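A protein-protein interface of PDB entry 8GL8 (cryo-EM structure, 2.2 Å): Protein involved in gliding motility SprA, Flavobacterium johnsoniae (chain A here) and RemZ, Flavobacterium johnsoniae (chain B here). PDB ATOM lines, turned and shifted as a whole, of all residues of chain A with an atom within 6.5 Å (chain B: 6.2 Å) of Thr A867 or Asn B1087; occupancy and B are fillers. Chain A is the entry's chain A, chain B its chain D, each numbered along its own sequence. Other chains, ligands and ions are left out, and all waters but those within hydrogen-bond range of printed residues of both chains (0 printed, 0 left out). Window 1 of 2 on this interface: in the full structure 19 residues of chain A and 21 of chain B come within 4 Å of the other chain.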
ATOM      1  N   GLN A 865     -23.390  -9.247 -23.854  1.00  0.00           N
ATOM      2  CA  GLN A 865     -23.357  -8.166 -22.869  1.00  0.00           C
ATOM      3  C   GLN A 865     -24.233  -6.983 -23.299  1.00  0.00           C
ATOM      4  O   GLN A 865     -23.757  -5.879 -23.576  1.00  0.00           O
ATOM      5  CB  GLN A 865     -21.915  -7.719 -22.610  1.00  0.00           C
ATOM      6  CG  GLN A 865     -20.980  -8.862 -22.278  1.00  0.00           C
ATOM      7  CD  GLN A 865     -20.641  -8.922 -20.807  1.00  0.00           C
ATOM      8  OE1 GLN A 865     -20.198  -7.935 -20.225  1.00  0.00           O
ATOM      9  NE2 GLN A 865     -20.848 -10.082 -20.197  1.00  0.00           N
ATOM     10  N   SER A 866     -25.534  -7.246 -23.351  1.00  0.00           N
ATOM     11  CA  SER A 866     -26.506  -6.176 -23.521  1.00  0.00           C
ATOM     12  C   SER A 866     -26.686  -5.414 -22.212  1.00  0.00           C
ATOM     13  O   SER A 866     -26.586  -5.985 -21.121  1.00  0.00           O
ATOM     14  CB  SER A 866     -27.846  -6.731 -24.005  1.00  0.00           C
ATOM     15  OG  SER A 866     -28.130  -7.982 -23.412  1.00  0.00           O
ATOM     16  N   THR A 867     -26.950  -4.117 -22.324  1.00  0.00           N
ATOM     17  CA  THR A 867     -27.030  -3.240 -21.165  1.00  0.00           C
ATOM     18  C   THR A 867     -28.439  -2.690 -20.993  1.00  0.00           C
ATOM     19  O   THR A 867     -29.179  -2.508 -21.963  1.00  0.00           O
ATOM     20  CB  THR A 867     -26.041  -2.073 -21.284  1.00  0.00           C
ATOM     21  OG1 THR A 867     -26.196  -1.436 -22.557  1.00  0.00           O
ATOM     22  CG2 THR A 867     -24.611  -2.568 -21.147  1.00  0.00           C
ATOM     23  N   ILE A 868     -28.801  -2.434 -19.740  1.00  0.00           N
ATOM     24  CA  ILE A 868     -30.041  -1.756 -19.383  1.00  0.00           C
ATOM     25  C   ILE A 868     -29.648  -0.502 -18.616  1.00  0.00           C
ATOM     26  O   ILE A 868     -29.050  -0.590 -17.538  1.00  0.00           O
ATOM     27  CB  ILE A 868     -30.972  -2.647 -18.550  1.00  0.00           C
ATOM     28  CG1 ILE A 868     -31.195  -3.990 -19.245  1.00  0.00           C
ATOM     29  CG2 ILE A 868     -32.302  -1.954 -18.320  1.00  0.00           C
ATOM     30  CD1 ILE A 868     -31.403  -5.140 -18.290  1.00  0.00           C
ATOM     31  N   ASP A 869     -29.982   0.660 -19.171  1.00  0.00           N
ATOM     32  CA  ASP A 869     -29.555   1.931 -18.600  1.00  0.00           C
ATOM     33  C   ASP A 869     -30.306   2.237 -17.310  1.00  0.00           C
ATOM     34  O   ASP A 869     -31.521   2.047 -17.217  1.00  0.00           O
ATOM     35  CB  ASP A 869     -29.773   3.054 -19.612  1.00  0.00           C
ATOM     36  CG  ASP A 869     -28.857   4.236 -19.379  1.00  0.00           C
ATOM     37  OD1 ASP A 869     -27.970   4.141 -18.506  1.00  0.00           O
ATOM     38  OD2 ASP A 869     -29.023   5.260 -20.071  1.00  0.00           O
ATOM     39  N   MET A 870     -29.571   2.731 -16.311  1.00  0.00           N
ATOM     40  CA  MET A 870     -30.136   3.068 -15.010  1.00  0.00           C
ATOM     41  C   MET A 870     -29.894   4.515 -14.600  1.00  0.00           C
ATOM     42  O   MET A 870     -30.223   4.882 -13.468  1.00  0.00           O
ATOM     43  CB  MET A 870     -29.579   2.137 -13.928  1.00  0.00           C
ATOM     44  CG  MET A 870     -29.827   0.665 -14.171  1.00  0.00           C
ATOM     45  SD  MET A 870     -31.463   0.180 -13.592  1.00  0.00           S
ATOM     46  CE  MET A 870     -32.202  -0.402 -15.107  1.00  0.00           C
ATOM     47  N   GLN A1008     -22.477  -2.238 -14.032  1.00  0.00           N
ATOM     48  CA  GLN A1008     -21.355  -1.525 -14.623  1.00  0.00           C
ATOM     49  C   GLN A1008     -21.602  -0.029 -14.515  1.00  0.00           C
ATOM     50  O   GLN A1008     -22.706   0.443 -14.798  1.00  0.00           O
ATOM     51  CB  GLN A1008     -21.163  -1.929 -16.086  1.00  0.00           C
ATOM     52  CG  GLN A1008     -19.815  -1.554 -16.664  1.00  0.00           C
ATOM     53  CD  GLN A1008     -19.737  -1.806 -18.156  1.00  0.00           C
ATOM     54  OE1 GLN A1008     -19.799  -2.948 -18.609  1.00  0.00           O
ATOM     55  NE2 GLN A1008     -19.598  -0.737 -18.930  1.00  0.00           N
ATOM     56  N   ASP A1258     -25.339   0.979 -15.808  1.00  0.00           N
ATOM     57  CA  ASP A1258     -26.129  -0.037 -16.481  1.00  0.00           C
ATOM     58  C   ASP A1258     -26.128  -1.337 -15.692  1.00  0.00           C
ATOM     59  O   ASP A1258     -25.199  -1.635 -14.934  1.00  0.00           O
ATOM     60  CB  ASP A1258     -25.601  -0.324 -17.897  1.00  0.00           C
ATOM     61  CG  ASP A1258     -25.239   0.936 -18.655  1.00  0.00           C
ATOM     62  OD1 ASP A1258     -26.072   1.863 -18.701  1.00  0.00           O
ATOM     63  OD2 ASP A1258     -24.117   0.999 -19.201  1.00  0.00           O
ATOM     64  N   LEU A1259     -27.196  -2.103 -15.880  1.00  0.00           N
ATOM     65  CA  LEU A1259     -27.208  -3.520 -15.549  1.00  0.00           C
ATOM     66  C   LEU A1259     -26.830  -4.288 -16.809  1.00  0.00           C
ATOM     67  O   LEU A1259     -27.508  -4.173 -17.834  1.00  0.00           O
ATOM     68  CB  LEU A1259     -28.580  -3.952 -15.039  1.00  0.00           C
ATOM     69  CG  LEU A1259     -28.971  -3.495 -13.633  1.00  0.00           C
ATOM     70  CD1 LEU A1259     -30.419  -3.845 -13.343  1.00  0.00           C
ATOM     71  CD2 LEU A1259     -28.052  -4.109 -12.597  1.00  0.00           C
ATOM     72  N   VAL A1260     -25.742  -5.048 -16.747  1.00  0.00           N
ATOM     73  CA  VAL A1260     -25.199  -5.734 -17.911  1.00  0.00           C
ATOM     74  C   VAL A1260     -25.526  -7.212 -17.790  1.00  0.00           C
ATOM     75  O   VAL A1260     -25.181  -7.856 -16.788  1.00  0.00           O
ATOM     76  CB  VAL A1260     -23.685  -5.515 -18.046  1.00  0.00           C
ATOM     77  CG1 VAL A1260     -23.172  -6.182 -19.308  1.00  0.00           C
ATOM     78  CG2 VAL A1260     -23.368  -4.033 -18.048  1.00  0.00           C
ATOM     79  N   ARG A1261     -26.188  -7.740 -18.817  1.00  0.00           N
ATOM     80  CA  ARG A1261     -26.514  -9.151 -18.925  1.00  0.00           C
ATOM     81  C   ARG A1261     -25.751  -9.757 -20.095  1.00  0.00           C
ATOM     82  O   ARG A1261     -25.541  -9.100 -21.119  1.00  0.00           O
ATOM     83  CB  ARG A1261     -28.022  -9.355 -19.105  1.00  0.00           C
ATOM     84  CG  ARG A1261     -28.586  -8.810 -20.400  1.00  0.00           C
ATOM     85  CD  ARG A1261     -30.034  -8.385 -20.238  1.00  0.00           C
ATOM     86  NE  ARG A1261     -30.955  -9.492 -20.463  1.00  0.00           N
ATOM     87  CZ  ARG A1261     -31.277  -9.972 -21.658  1.00  0.00           C
ATOM     88  NH1 ARG A1261     -30.784  -9.451 -22.769  1.00  0.00           N
ATOM     89  NH2 ARG A1261     -32.115 -11.001 -21.739  1.00  0.00           N
ATOM     90  N   ASP B1047     -39.797   3.314 -21.385  1.00  0.00           N
ATOM     91  CA  ASP B1047     -38.446   3.490 -20.844  1.00  0.00           C
ATOM     92  C   ASP B1047     -37.549   2.451 -21.515  1.00  0.00           C
ATOM     93  O   ASP B1047     -37.296   1.375 -20.968  1.00  0.00           O
ATOM     94  CB  ASP B1047     -38.423   3.354 -19.322  1.00  0.00           C
ATOM     95  CG  ASP B1047     -39.685   3.881 -18.666  1.00  0.00           C
ATOM     96  OD1 ASP B1047     -39.955   5.094 -18.779  1.00  0.00           O
ATOM     97  OD2 ASP B1047     -40.406   3.079 -18.038  1.00  0.00           O
ATOM     98  N   LYS B1048     -37.052   2.794 -22.704  1.00  0.00           N
ATOM     99  CA  LYS B1048     -36.161   1.932 -23.483  1.00  0.00           C
ATOM    100  C   LYS B1048     -36.724   0.524 -23.672  1.00  0.00           C
ATOM    101  O   LYS B1048     -35.969  -0.431 -23.881  1.00  0.00           O
ATOM    102  CB  LYS B1048     -34.768   1.868 -22.849  1.00  0.00           C
ATOM    103  CG  LYS B1048     -34.007   3.181 -22.901  1.00  0.00           C
ATOM    104  CD  LYS B1048     -33.377   3.390 -24.267  1.00  0.00           C
ATOM    105  CE  LYS B1048     -32.153   4.284 -24.184  1.00  0.00           C
ATOM    106  NZ  LYS B1048     -32.348   5.550 -24.939  1.00  0.00           N
ATOM    107  N   THR B1049     -38.044   0.374 -23.601  1.00  0.00           N
ATOM    108  CA  THR B1049     -38.710  -0.909 -23.775  1.00  0.00           C
ATOM    109  C   THR B1049     -39.751  -0.774 -24.875  1.00  0.00           C
ATOM    110  O   THR B1049     -40.561   0.158 -24.853  1.00  0.00           O
ATOM    111  CB  THR B1049     -39.368  -1.373 -22.473  1.00  0.00           C
ATOM    112  OG1 THR B1049     -38.408  -1.347 -21.412  1.00  0.00           O
ATOM    113  CG2 THR B1049     -39.903  -2.784 -22.624  1.00  0.00           C
ATOM    114  N   GLN B1084     -36.694  -5.840 -24.969  1.00  0.00           N
ATOM    115  CA  GLN B1084     -35.624  -5.069 -24.344  1.00  0.00           C
ATOM    116  C   GLN B1084     -34.404  -5.141 -25.256  1.00  0.00           C
ATOM    117  O   GLN B1084     -33.662  -6.127 -25.239  1.00  0.00           O
ATOM    118  CB  GLN B1084     -35.308  -5.604 -22.950  1.00  0.00           C
ATOM    119  CG  GLN B1084     -35.861  -4.768 -21.808  1.00  0.00           C
ATOM    120  CD  GLN B1084     -35.247  -5.136 -20.469  1.00  0.00           C
ATOM    121  OE1 GLN B1084     -34.778  -6.259 -20.275  1.00  0.00           O
ATOM    122  NE2 GLN B1084     -35.246  -4.189 -19.536  1.00  0.00           N
ATOM    123  N   VAL B1085     -34.205  -4.104 -26.052  1.00  0.00           N
ATOM    124  CA  VAL B1085     -33.025  -3.984 -26.898  1.00  0.00           C
ATOM    125  C   VAL B1085     -31.937  -3.296 -26.085  1.00  0.00           C
ATOM    126  O   VAL B1085     -32.224  -2.570 -25.127  1.00  0.00           O
ATOM    127  CB  VAL B1085     -33.354  -3.214 -28.196  1.00  0.00           C
ATOM    128  CG1 VAL B1085     -32.208  -3.303 -29.193  1.00  0.00           C
ATOM    129  CG2 VAL B1085     -34.638  -3.743 -28.812  1.00  0.00           C
ATOM    130  N   SER B1086     -30.678  -3.540 -26.451  1.00  0.00           N
ATOM    131  CA  SER B1086     -29.559  -2.936 -25.739  1.00  0.00           C
ATOM    132  C   SER B1086     -29.700  -1.420 -25.723  1.00  0.00           C
ATOM    133  O   SER B1086     -29.948  -0.794 -26.758  1.00  0.00           O
ATOM    134  CB  SER B1086     -28.237  -3.346 -26.387  1.00  0.00           C
ATOM    135  OG  SER B1086     -27.148  -3.129 -25.507  1.00  0.00           O
ATOM    136  N   ASN B1087     -29.543  -0.830 -24.537  1.00  0.00           N
ATOM    137  CA  ASN B1087     -29.895   0.572 -24.349  1.00  0.00           C
ATOM    138  C   ASN B1087     -28.882   1.520 -24.978  1.00  0.00           C
ATOM    139  O   ASN B1087     -29.247   2.638 -25.360  1.00  0.00           O
ATOM    140  CB  ASN B1087     -30.051   0.877 -22.858  1.00  0.00           C
ATOM    141  CG  ASN B1087     -31.390   0.418 -22.306  1.00  0.00           C
ATOM    142  OD1 ASN B1087     -31.857   0.919 -21.284  1.00  0.00           O
ATOM    143  ND2 ASN B1087     -32.015  -0.537 -22.983  1.00  0.00           N
ATOM    144  N   PHE B1088     -27.624   1.107 -25.099  1.00  0.00           N
ATOM    145  CA  PHE B1088     -26.604   1.954 -25.704  1.00  0.00           C
ATOM    146  C   PHE B1088     -26.610   1.754 -27.215  1.00  0.00           C
ATOM    147  O   PHE B1088     -26.359   0.647 -27.702  1.00  0.00           O
ATOM    148  CB  PHE B1088     -25.228   1.635 -25.120  1.00  0.00           C
ATOM    149  CG  PHE B1088     -24.157   2.605 -25.532  1.00  0.00           C
ATOM    150  CD1 PHE B1088     -23.429   2.405 -26.695  1.00  0.00           C
ATOM    151  CD2 PHE B1088     -23.877   3.718 -24.756  1.00  0.00           C
ATOM    152  CE1 PHE B1088     -22.445   3.295 -27.076  1.00  0.00           C
ATOM    153  CE2 PHE B1088     -22.892   4.612 -25.132  1.00  0.00           C
ATOM    154  CZ  PHE B1088     -22.176   4.400 -26.294  1.00  0.00           C
ATOM    155  N   GLN B1089     -26.893   2.828 -27.957  1.00  0.00           N
ATOM    156  CA  GLN B1089     -26.957   2.765 -29.413  1.00  0.00           C
ATOM    157  C   GLN B1089     -26.141   3.872 -30.073  1.00  0.00           C
ATOM    158  O   GLN B1089     -26.333   4.148 -31.261  1.00  0.00           O
ATOM    159  CB  GLN B1089     -28.408   2.817 -29.895  1.00  0.00           C
ATOM    160  CG  GLN B1089     -29.208   1.555 -29.603  1.00  0.00           C
ATOM    161  CD  GLN B1089     -28.612   0.318 -30.249  1.00  0.00           C
ATOM    162  OE1 GLN B1089     -28.006   0.389 -31.318  1.00  0.00           O
ATOM    163  NE2 GLN B1089     -28.782  -0.827 -29.600  1.00  0.00           N
ATOM    164  N   SER B1090     -25.241   4.512 -29.322  1.00  0.00           N
ATOM    165  CA  SER B1090     -24.312   5.513 -29.850  1.00  0.00           C
ATOM    166  C   SER B1090     -25.055   6.682 -30.504  1.00  0.00           C
ATOM    167  O   SER B1090     -24.880   6.985 -31.686  1.00  0.00           O
ATOM    168  CB  SER B1090     -23.317   4.875 -30.826  1.00  0.00           C
ATOM    169  OG  SER B1090     -22.822   3.649 -30.322  1.00  0.00           O
ATOM    170  N   PHE B1113     -36.454   5.688 -29.956  1.00  0.00           N
ATOM    171  CA  PHE B1113     -36.036   4.909 -28.795  1.00  0.00           C
ATOM    172  C   PHE B1113     -35.755   5.855 -27.635  1.00  0.00           C
ATOM    173  O   PHE B1113     -34.746   6.566 -27.634  1.00  0.00           O
ATOM    174  CB  PHE B1113     -34.807   4.072 -29.135  1.00  0.00           C
ATOM    175  CG  PHE B1113     -34.651   2.849 -28.280  1.00  0.00           C
ATOM    176  CD1 PHE B1113     -35.756   2.116 -27.890  1.00  0.00           C
ATOM    177  CD2 PHE B1113     -33.396   2.432 -27.872  1.00  0.00           C
ATOM    178  CE1 PHE B1113     -35.615   0.989 -27.104  1.00  0.00           C
ATOM    179  CE2 PHE B1113     -33.247   1.305 -27.088  1.00  0.00           C
ATOM    180  CZ  PHE B1113     -34.358   0.583 -26.703  1.00  0.00           C
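Of the printed residues of chain B, Ser A866 touches Ser B1086. Of the printed residues of chain B, Thr A867 touches Ser B1086, Asn B1087 and Phe B1088. Printed residues of chain B within 4 Å of Asp A869: Asn B1087. Of the printed residues of chain A, Asn B1087 touches Thr A867, Ile A868 and Asp A869. The nearest printed residue of chain B that does not touch Thr A867 is Val B1085 (4.4 Å). The nearest printed residue of chain A that does not touch Asn B1087 is Met A870 (5.8 Å). The nearest printed residue of chain A that does not touch Phe B1088 is Asp A1258 (6.1 Å).
The backbone NH of Asp A869 sits at hydrogen-bond distance from the side-chain amide oxygen of Asn B1087, 2.8 Å away. N of Thr A867 lies within hydrogen-bond range of OG of Ser B1086 (3.3 Å). O of Thr A867 lies within hydrogen-bond range of N of Asn B1087.
Among the printed residues, merely in contact across the chains: Ser A866 with Ser B1086 (3.7 Å), Thr A867 with Phe B1088 (3.9 Å), Ile A868 with Gln B1084 (3.9 Å) and Ile A868 with Asn B1087 (3.7 Å).
The side-chain amide nitrogen of Asn B1087 is in hydrogen-bond range of the backbone carbonyl oxygen of Val B1085 (3.0 Å). N of Ser A866 is in hydrogen-bond range of O of Arg A1261, at 2.9 Å. The backbone carbonyl oxygen (O) of Leu A1259 sits at hydrogen-bond distance from the backbone NH (N) of Ile A868 (2.9 Å). NE2 of Gln B1089 sits at hydrogen-bond distance from O of Ser B1086 (3.1 Å).
Of the 11 printed residues of chain B, 4 touch a printed residue of chain A. Printed residues of chain B that touch a printed residue of chain A: Gln B1084, Ser B1086, Asn B1087 and Phe B1088. Of the 11 printed residues of chain A, 4 touch a printed residue of chain B. Printed residues of chain A that touch a printed residue of chain B: Ser A866, Thr A867, Ile A868 and Asp A869. Among the printed residues, 7 pairs touch across the chains.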
